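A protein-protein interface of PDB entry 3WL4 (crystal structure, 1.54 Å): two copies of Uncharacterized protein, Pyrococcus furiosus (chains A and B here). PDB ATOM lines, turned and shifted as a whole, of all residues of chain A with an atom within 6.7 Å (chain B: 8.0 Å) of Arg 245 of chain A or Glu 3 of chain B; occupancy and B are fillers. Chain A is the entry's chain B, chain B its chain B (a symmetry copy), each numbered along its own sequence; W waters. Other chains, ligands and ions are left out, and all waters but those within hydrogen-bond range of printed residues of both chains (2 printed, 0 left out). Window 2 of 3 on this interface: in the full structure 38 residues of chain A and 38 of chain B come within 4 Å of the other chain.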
ATOM      1  N   ASP A 200       8.999  10.421 -11.401  1.00  0.00           N
ATOM      2  CA  ASP A 200      10.102  10.761 -10.457  1.00  0.00           C
ATOM      3  C   ASP A 200      10.387   9.514  -9.660  1.00  0.00           C
ATOM      4  O   ASP A 200       9.465   8.924  -9.015  1.00  0.00           O
ATOM      5  CB  ASP A 200       9.533  11.884  -9.543  1.00  0.00           C
ATOM      6  CG  ASP A 200      10.516  12.283  -8.464  1.00  0.00           C
ATOM      7  OD1 ASP A 200      11.631  11.805  -8.460  1.00  0.00           O
ATOM      8  OD2 ASP A 200      10.111  13.192  -7.660  1.00  0.00           O
ATOM      9  N   THR A 202      13.252   9.531  -7.658  1.00  0.00           N
ATOM     10  CA  THR A 202      14.348   9.943  -6.720  1.00  0.00           C
ATOM     11  C   THR A 202      14.414   9.101  -5.445  1.00  0.00           C
ATOM     12  O   THR A 202      15.528   8.623  -5.075  1.00  0.00           O
ATOM     13  CB  THR A 202      14.061  11.401  -6.400  1.00  0.00           C
ATOM     14  OG1 THR A 202      14.220  12.184  -7.557  1.00  0.00           O
ATOM     15  CG2 THR A 202      15.187  11.893  -5.423  1.00  0.00           C
ATOM     16  N   GLU A 206      18.085   3.994  -5.057  1.00  0.00           N
ATOM     17  CA  GLU A 206      18.921   2.979  -4.499  1.00  0.00           C
ATOM     18  C   GLU A 206      18.338   1.536  -4.667  1.00  0.00           C
ATOM     19  O   GLU A 206      19.077   0.636  -4.920  1.00  0.00           O
ATOM     20  CB  GLU A 206      19.179   3.278  -2.934  1.00  0.00           C
ATOM     21  CG  GLU A 206      20.054   4.566  -2.785  1.00  0.00           C
ATOM     22  CD  GLU A 206      21.468   4.525  -3.510  1.00  0.00           C
ATOM     23  OE1 GLU A 206      22.307   3.534  -3.433  1.00  0.00           O
ATOM     24  OE2 GLU A 206      21.662   5.511  -4.199  1.00  0.00           O
ATOM     25  N   GLU A 228      27.379   2.615 -12.993  1.00  0.00           N
ATOM     26  CA  GLU A 228      26.686   3.547 -12.091  1.00  0.00           C
ATOM     27  C   GLU A 228      26.726   4.950 -12.584  1.00  0.00           C
ATOM     28  O   GLU A 228      25.677   5.607 -12.576  1.00  0.00           O
ATOM     29  CB  GLU A 228      27.095   3.261 -10.566  1.00  0.00           C
ATOM     30  CG  GLU A 228      26.259   4.142  -9.715  1.00  0.00           C
ATOM     31  CD  GLU A 228      26.594   4.030  -8.213  1.00  0.00           C
ATOM     32  OE1 GLU A 228      26.096   4.877  -7.449  1.00  0.00           O
ATOM     33  OE2 GLU A 228      27.080   2.979  -7.783  1.00  0.00           O
ATOM     34  N   ARG A 232      23.218   6.912 -13.392  1.00  0.00           N
ATOM     35  CA  ARG A 232      22.827   8.134 -12.792  1.00  0.00           C
ATOM     36  C   ARG A 232      22.758   9.299 -13.798  1.00  0.00           C
ATOM     37  O   ARG A 232      21.857  10.136 -13.630  1.00  0.00           O
ATOM     38  CB  ARG A 232      23.940   8.560 -11.733  1.00  0.00           C
ATOM     39  CG  ARG A 232      24.058   7.527 -10.637  1.00  0.00           C
ATOM     40  CD  ARG A 232      24.069   8.202  -9.255  1.00  0.00           C
ATOM     41  NE  ARG A 232      24.281   7.183  -8.198  1.00  0.00           N
ATOM     42  CZ  ARG A 232      23.418   6.978  -7.185  1.00  0.00           C
ATOM     43  NH1 ARG A 232      22.387   7.781  -7.006  1.00  0.00           N
ATOM     44  NH2 ARG A 232      23.769   6.014  -6.325  1.00  0.00           N
ATOM     45  N   THR A 235      19.334   8.873 -15.532  1.00  0.00           N
ATOM     46  CA  THR A 235      18.153   9.251 -14.674  1.00  0.00           C
ATOM     47  C   THR A 235      18.118  10.785 -14.391  1.00  0.00           C
ATOM     48  O   THR A 235      17.067  11.322 -14.264  1.00  0.00           O
ATOM     49  CB  THR A 235      18.156   8.483 -13.303  1.00  0.00           C
ATOM     50  OG1 THR A 235      19.392   8.670 -12.683  1.00  0.00           O
ATOM     51  CG2 THR A 235      18.276   6.971 -13.724  1.00  0.00           C
ATOM     52  N   MET A 236      19.286  11.447 -14.419  1.00  0.00           N
ATOM     53  CA  MET A 236      19.310  12.927 -14.319  1.00  0.00           C
ATOM     54  C   MET A 236      18.778  13.556 -15.587  1.00  0.00           C
ATOM     55  O   MET A 236      18.074  14.542 -15.618  1.00  0.00           O
ATOM     56  CB  MET A 236      20.723  13.431 -13.984  1.00  0.00           C
ATOM     57  CG  MET A 236      21.037  12.858 -12.648  1.00  0.00           C
ATOM     58  SD  MET A 236      22.956  13.376 -12.166  1.00  0.00           S
ATOM     59  CE  MET A 236      22.565  15.172 -12.026  1.00  0.00           C
ATOM     60  N   PHE A 237      19.146  12.957 -16.736  1.00  0.00           N
ATOM     61  CA  PHE A 237      18.617  13.429 -18.010  1.00  0.00           C
ATOM     62  C   PHE A 237      17.097  13.473 -17.999  1.00  0.00           C
ATOM     63  O   PHE A 237      16.537  14.482 -18.388  1.00  0.00           O
ATOM     64  CB  PHE A 237      19.130  12.447 -19.128  1.00  0.00           C
ATOM     65  CG  PHE A 237      18.549  12.688 -20.525  1.00  0.00           C
ATOM     66  CD1 PHE A 237      19.047  13.706 -21.312  1.00  0.00           C
ATOM     67  CD2 PHE A 237      17.503  11.897 -20.993  1.00  0.00           C
ATOM     68  CE1 PHE A 237      18.529  13.890 -22.610  1.00  0.00           C
ATOM     69  CE2 PHE A 237      16.948  12.090 -22.258  1.00  0.00           C
ATOM     70  CZ  PHE A 237      17.528  13.084 -23.120  1.00  0.00           C
ATOM     71  N   TYR A 238      16.477  12.406 -17.521  1.00  0.00           N
ATOM     72  CA  TYR A 238      15.026  12.401 -17.408  1.00  0.00           C
ATOM     73  C   TYR A 238      14.466  13.274 -16.299  1.00  0.00           C
ATOM     74  O   TYR A 238      13.534  14.062 -16.518  1.00  0.00           O
ATOM     75  CB  TYR A 238      14.466  10.963 -17.290  1.00  0.00           C
ATOM     76  CG  TYR A 238      14.745  10.095 -18.495  1.00  0.00           C
ATOM     77  CD1 TYR A 238      14.256  10.498 -19.736  1.00  0.00           C
ATOM     78  CD2 TYR A 238      15.396   8.940 -18.339  1.00  0.00           C
ATOM     79  CE1 TYR A 238      14.512   9.635 -20.863  1.00  0.00           C
ATOM     80  CE2 TYR A 238      15.653   8.069 -19.441  1.00  0.00           C
ATOM     81  CZ  TYR A 238      15.146   8.481 -20.665  1.00  0.00           C
ATOM     82  OH  TYR A 238      15.412   7.617 -21.778  1.00  0.00           O
ATOM     83  N   GLY A 239      15.123  13.112 -15.139  1.00  0.00           N
ATOM     84  CA  GLY A 239      14.555  13.907 -13.976  1.00  0.00           C
ATOM     85  C   GLY A 239      14.633  15.437 -14.226  1.00  0.00           C
ATOM     86  O   GLY A 239      13.647  16.116 -13.839  1.00  0.00           O
ATOM     87  N   GLU A 240      15.716  15.908 -14.853  1.00  0.00           N
ATOM     88  CA  GLU A 240      15.839  17.388 -15.066  1.00  0.00           C
ATOM     89  C   GLU A 240      14.667  17.923 -15.870  1.00  0.00           C
ATOM     90  O   GLU A 240      14.244  19.084 -15.641  1.00  0.00           O
ATOM     91  CB  GLU A 240      17.125  17.684 -15.709  1.00  0.00           C
ATOM     92  CG  GLU A 240      17.519  19.161 -15.592  1.00  0.00           C
ATOM     93  CD  GLU A 240      18.998  19.313 -15.872  1.00  0.00           C
ATOM     94  OE1 GLU A 240      19.848  18.935 -14.982  1.00  0.00           O
ATOM     95  OE2 GLU A 240      19.334  19.739 -17.009  1.00  0.00           O
ATOM     96  N   GLY A 243      12.136  18.746 -13.386  1.00  0.00           N
ATOM     97  CA  GLY A 243      12.642  19.496 -12.139  1.00  0.00           C
ATOM     98  C   GLY A 243      12.883  18.595 -10.929  1.00  0.00           C
ATOM     99  O   GLY A 243      12.758  19.032  -9.739  1.00  0.00           O
ATOM    100  N   VAL A 244      13.166  17.292 -11.084  1.00  0.00           N
ATOM    101  CA  VAL A 244      13.444  16.351 -10.037  1.00  0.00           C
ATOM    102  C   VAL A 244      14.847  15.731 -10.232  1.00  0.00           C
ATOM    103  O   VAL A 244      15.436  15.833 -11.289  1.00  0.00           O
ATOM    104  CB  VAL A 244      12.376  15.238  -9.809  1.00  0.00           C
ATOM    105  CG1 VAL A 244      10.981  15.765  -9.665  1.00  0.00           C
ATOM    106  CG2 VAL A 244      12.402  14.113 -10.988  1.00  0.00           C
ATOM    107  N   ARG A 245      15.387  15.153  -9.168  1.00  0.00           N
ATOM    108  CA  ARG A 245      16.736  14.634  -9.239  1.00  0.00           C
ATOM    109  C   ARG A 245      16.834  13.451 -10.285  1.00  0.00           C
ATOM    110  O   ARG A 245      17.710  13.513 -11.143  1.00  0.00           O
ATOM    111  CB  ARG A 245      17.274  14.164  -7.875  1.00  0.00           C
ATOM    112  CG  ARG A 245      18.799  13.983  -7.894  1.00  0.00           C
ATOM    113  CD  ARG A 245      19.282  13.522  -6.521  1.00  0.00           C
ATOM    114  NE  ARG A 245      20.729  13.467  -6.540  1.00  0.00           N
ATOM    115  CZ  ARG A 245      21.438  12.791  -5.566  1.00  0.00           C
ATOM    116  NH1 ARG A 245      20.853  12.084  -4.567  1.00  0.00           N
ATOM    117  NH2 ARG A 245      22.803  12.792  -5.608  1.00  0.00           N
ATOM    118  N   TYR A 246      15.994  12.439 -10.045  1.00  0.00           N
ATOM    119  CA  TYR A 246      16.142  11.190 -10.871  1.00  0.00           C
ATOM    120  C   TYR A 246      14.715  10.894 -11.377  1.00  0.00           C
ATOM    121  O   TYR A 246      13.738  10.809 -10.674  1.00  0.00           O
ATOM    122  CB  TYR A 246      16.551  10.047  -9.977  1.00  0.00           C
ATOM    123  CG  TYR A 246      17.946  10.223  -9.403  1.00  0.00           C
ATOM    124  CD1 TYR A 246      19.030  10.647 -10.199  1.00  0.00           C
ATOM    125  CD2 TYR A 246      18.153   9.886  -8.096  1.00  0.00           C
ATOM    126  CE1 TYR A 246      20.365  10.740  -9.655  1.00  0.00           C
ATOM    127  CE2 TYR A 246      19.498   9.930  -7.547  1.00  0.00           C
ATOM    128  CZ  TYR A 246      20.525  10.410  -8.290  1.00  0.00           C
ATOM    129  OH  TYR A 246      21.820  10.505  -7.859  1.00  0.00           O
ATOM    130  N   GLY A 247      14.750  10.599 -12.689  1.00  0.00           N
ATOM    131  CA  GLY A 247      13.476  10.305 -13.401  1.00  0.00           C
ATOM    132  C   GLY A 247      13.661   9.098 -14.350  1.00  0.00           C
ATOM    133  O   GLY A 247      14.754   8.733 -14.712  1.00  0.00           O
ATOM    134  N   MET B   1      28.488   6.596  -6.560  1.00  0.00           N
ATOM    135  CA  MET B   1      29.219   7.359  -7.588  1.00  0.00           C
ATOM    136  C   MET B   1      28.276   8.301  -8.324  1.00  0.00           C
ATOM    137  O   MET B   1      27.091   7.969  -8.438  1.00  0.00           O
ATOM    138  CB  MET B   1      29.797   6.387  -8.635  1.00  0.00           C
ATOM    139  CG  MET B   1      30.999   5.552  -7.969  1.00  0.00           C
ATOM    140  SD  MET B   1      31.670   4.204  -9.176  1.00  0.00           S
ATOM    141  CE  MET B   1      30.383   2.798  -8.743  1.00  0.00           C
ATOM    142  N   PHE B   2      28.859   9.432  -8.836  1.00  0.00           N
ATOM    143  CA  PHE B   2      28.024  10.399  -9.511  1.00  0.00           C
ATOM    144  C   PHE B   2      26.904  10.913  -8.722  1.00  0.00           C
ATOM    145  O   PHE B   2      25.850  11.370  -9.225  1.00  0.00           O
ATOM    146  CB  PHE B   2      27.557   9.825 -10.922  1.00  0.00           C
ATOM    147  CG  PHE B   2      28.464  10.152 -12.025  1.00  0.00           C
ATOM    148  CD1 PHE B   2      27.916  10.739 -13.206  1.00  0.00           C
ATOM    149  CD2 PHE B   2      29.877   9.847 -12.002  1.00  0.00           C
ATOM    150  CE1 PHE B   2      28.732  10.947 -14.253  1.00  0.00           C
ATOM    151  CE2 PHE B   2      30.745  10.107 -13.026  1.00  0.00           C
ATOM    152  CZ  PHE B   2      30.170  10.698 -14.254  1.00  0.00           C
ATOM    153  N   GLU B   3      27.145  11.027  -7.424  1.00  0.00           N
ATOM    154  CA  GLU B   3      26.164  11.585  -6.455  1.00  0.00           C
ATOM    155  C   GLU B   3      26.401  13.061  -6.207  1.00  0.00           C
ATOM    156  O   GLU B   3      25.423  13.753  -5.850  1.00  0.00           O
ATOM    157  CB  GLU B   3      26.205  10.776  -5.146  1.00  0.00           C
ATOM    158  CG  GLU B   3      25.544   9.400  -5.408  1.00  0.00           C
ATOM    159  CD  GLU B   3      25.809   8.537  -4.312  1.00  0.00           C
ATOM    160  OE1 GLU B   3      26.884   7.872  -4.337  1.00  0.00           O
ATOM    161  OE2 GLU B   3      24.952   8.461  -3.446  1.00  0.00           O
ATOM    162  N   ASN B   4      27.594  13.519  -6.575  1.00  0.00           N
ATOM    163  CA  ASN B   4      27.860  14.931  -6.275  1.00  0.00           C
ATOM    164  C   ASN B   4      27.656  15.923  -7.392  1.00  0.00           C
ATOM    165  O   ASN B   4      27.602  17.137  -7.174  1.00  0.00           O
ATOM    166  CB  ASN B   4      29.216  15.018  -5.556  1.00  0.00           C
ATOM    167  CG  ASN B   4      29.103  14.498  -4.087  1.00  0.00           C
ATOM    168  OD1 ASN B   4      27.990  14.121  -3.619  1.00  0.00           O
ATOM    169  ND2 ASN B   4      30.216  14.315  -3.449  1.00  0.00           N
ATOM    170  N   VAL B   5      27.430  15.463  -8.597  1.00  0.00           N
ATOM    171  CA  VAL B   5      26.946  16.360  -9.643  1.00  0.00           C
ATOM    172  C   VAL B   5      25.496  16.787  -9.461  1.00  0.00           C
ATOM    173  O   VAL B   5      24.671  16.001  -8.911  1.00  0.00           O
ATOM    174  CB  VAL B   5      27.196  15.638 -11.015  1.00  0.00           C
ATOM    175  CG1 VAL B   5      28.685  15.459 -11.269  1.00  0.00           C
ATOM    176  CG2 VAL B   5      26.547  14.231 -11.039  1.00  0.00           C
ATOM    177  N   SER B   6      25.161  17.981  -9.965  1.00  0.00           N
ATOM    178  CA  SER B   6      23.921  18.641  -9.703  1.00  0.00           C
ATOM    179  C   SER B   6      23.033  18.760 -10.891  1.00  0.00           C
ATOM    180  O   SER B   6      21.821  19.001 -10.686  1.00  0.00           O
ATOM    181  CB  SER B   6      24.288  20.128  -9.221  1.00  0.00           C
ATOM    182  OG  SER B   6      24.454  19.920  -7.886  1.00  0.00           O
ATOM    183  N   THR B   7      23.642  18.780 -12.055  1.00  0.00           N
ATOM    184  CA  THR B   7      22.834  18.980 -13.276  1.00  0.00           C
ATOM    185  C   THR B   7      23.188  17.880 -14.275  1.00  0.00           C
ATOM    186  O   THR B   7      24.278  17.308 -14.258  1.00  0.00           O
ATOM    187  CB  THR B   7      23.123  20.308 -13.976  1.00  0.00           C
ATOM    188  OG1 THR B   7      24.463  20.413 -14.414  1.00  0.00           O
ATOM    189  CG2 THR B   7      22.864  21.546 -12.991  1.00  0.00           C
ATOM    190  N   PHE B   8      22.243  17.699 -15.227  1.00  0.00           N
ATOM    191  CA  PHE B   8      22.556  16.720 -16.291  1.00  0.00           C
ATOM    192  C   PHE B   8      23.775  17.137 -17.073  1.00  0.00           C
ATOM    193  O   PHE B   8      24.646  16.345 -17.413  1.00  0.00           O
ATOM    194  CB  PHE B   8      21.306  16.597 -17.276  1.00  0.00           C
ATOM    195  CG  PHE B   8      21.728  15.869 -18.525  1.00  0.00           C
ATOM    196  CD1 PHE B   8      22.012  14.524 -18.495  1.00  0.00           C
ATOM    197  CD2 PHE B   8      21.873  16.591 -19.702  1.00  0.00           C
ATOM    198  CE1 PHE B   8      22.551  13.899 -19.675  1.00  0.00           C
ATOM    199  CE2 PHE B   8      22.393  16.004 -20.866  1.00  0.00           C
ATOM    200  CZ  PHE B   8      22.670  14.601 -20.847  1.00  0.00           C
ATOM    201  N   LYS B  14      31.113  14.988 -17.179  1.00  0.00           N
ATOM    202  CA  LYS B  14      31.954  14.124 -16.383  1.00  0.00           C
ATOM    203  C   LYS B  14      32.029  12.669 -16.889  1.00  0.00           C
ATOM    204  O   LYS B  14      33.051  11.996 -16.924  1.00  0.00           O
ATOM    205  CB  LYS B  14      31.516  14.187 -14.919  1.00  0.00           C
ATOM    206  CG  LYS B  14      32.404  13.422 -13.947  1.00  0.00           C
ATOM    207  CD  LYS B  14      31.710  13.499 -12.593  1.00  0.00           C
ATOM    208  CE  LYS B  14      32.477  12.692 -11.543  1.00  0.00           C
ATOM    209  NZ  LYS B  14      33.817  13.449 -11.171  1.00  0.00           N
HETATM  210  O   HOH W   1      23.379  12.295  -8.939  1.00  0.00           O
HETATM  211  O   HOH W   2      22.174  14.917  -8.122  1.00  0.00           O
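NH2 of Arg 232 of chain A lies within salt-bridge range of OE2 of Glu 3 of chain B, at 3.96 Å.
N of Phe 8 of chain B lies within hydrogen-bond range of OE1 of Glu 240 of chain A (2.7 Å).
The guanidinium group (NE) of Arg 232 of chain A is in hydrogen-bond range of the backbone carbonyl oxygen (O) of Met 1 of chain B.
OE1 of Glu 228 of chain A lies within hydrogen-bond range of N of Met 1 of chain B (3.1 Å).
The guanidinium group of Arg 245 of chain A lies within hydrogen-bond range of the backbone carbonyl oxygen of Glu 3 of chain B (2.8 Å).
OE1 of Glu 3 of chain B lies within hydrogen-bond range of N of Met 1 of chain B, 3.0 Å away.
O of Arg 232 of chain A sits at hydrogen-bond distance from OG1 of Thr 235 of chain A, at 3.0 Å.
The side-chain carboxylate (OE1) of Glu 228 of chain A lies within salt-bridge range of the guanidinium group (NH2) of Arg 232 of chain A.
The guanidinium group (NH2) of Arg 245 of chain A sits close to the side-chain hydroxyl (OH) of Tyr 246 of chain A, at 3.4 Å.
The guanidinium group (NH2) of Arg 232 of chain A lies within salt-bridge range of the side-chain carboxylate (OE2) of Glu 206 of chain A.
NH1 of Arg 232 of chain A lies within hydrogen-bond range of OH of Tyr 246 of chain A, 2.9 Å away.
Among the printed residues, pairs that only touch across the chains: Arg 232 of chain A with Phe 2 of chain B (3.6 Å), Met 236 of chain A with Val 5 of chain B (3.9 Å), Met 236 of chain A with Ser 6 of chain B (3.8 Å), Met 236 of chain A with Thr 7 of chain B (3.5 Å), Phe 237 of chain A with Phe 8 of chain B (3.6 Å) and Glu 240 of chain A with Thr 7 of chain B (3.4 Å).
Arg 245 of chain A touches just one residue of chain B: Glu 3.
Of chain A, only Arg 232 (3.7 Å) and Arg 245 (2.8 Å) come within 4 Å of Glu 3 of chain B.
Printed residues of chain A within 4 Å of Phe 2 of chain B: Arg 232.
Printed residues of chain B within 4 Å of Glu 240 of chain A: Thr 7 and Phe 8.
Printed residues of chain A within 4 Å of Thr 7 of chain B: Met 236 and Glu 240.
Of the printed residues of chain A, Ser 6 of chain B touches Met 236 (3.8 Å).
Printed residues of chain B within 4 Å of Met 236 of chain A: Val 5 (3.9 Å), Ser 6 (3.8 Å) and Thr 7 (3.5 Å).
Gly 243 of chain A touches none of the printed residues of chain B.
The nearest residue of chain A that does not touch Glu 3 of chain B is Glu 228 of chain A (4.4 Å).
The nearest printed residue of chain B that does not touch Met 236 of chain A is Phe 8 of chain B (4.1 Å).
Printed residues of chain B that touch a printed residue of chain A: Met 1, Phe 2, Glu 3, Val 5, Ser 6, Thr 7 and Phe 8.
Hydrophobic or aromatic side chains of chain B within 4 Å of the printed part of chain A: Met 1, Phe 2, Val 5 and Phe 8.
Printed residues of chain A that touch a printed residue of chain B: Glu 228, Arg 232, Met 236, Phe 237, Glu 240 and Arg 245.
Hydrophobic or aromatic side chains of chain A within 4 Å of the printed part of chain B: Met 236 and Phe 237.
Along chain A the printed residues that touch a printed residue of chain B span positions 228 to 245.
Among the printed residues, Asp or Glu carboxylates within 4 Å of a Lys or Arg side-chain nitrogen of the other chain: Arg 232 of chain A with Glu 3 of chain B (3.96 Å).
No position is printed for both chains.
Of the 11 pairs that touch across the chains among the printed residues, none has its exchanged pair printed and touching as well.
Water W2 lies within hydrogen-bond range of NE of Arg 245 of chain A and O of Val 5 of chain B.
Water W1 lies within hydrogen-bond range of the side-chain hydroxyl (OH) of Tyr 246 of chain A (2.6 Å), the backbone carbonyl oxygen (O) of Phe 2 of chain B (2.7 Å), the guanidinium group (NH2) of Arg 245 of chain A (3.4 Å) and the side-chain sulfur (SD) of Met 236 of chain A (3.4 Å).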
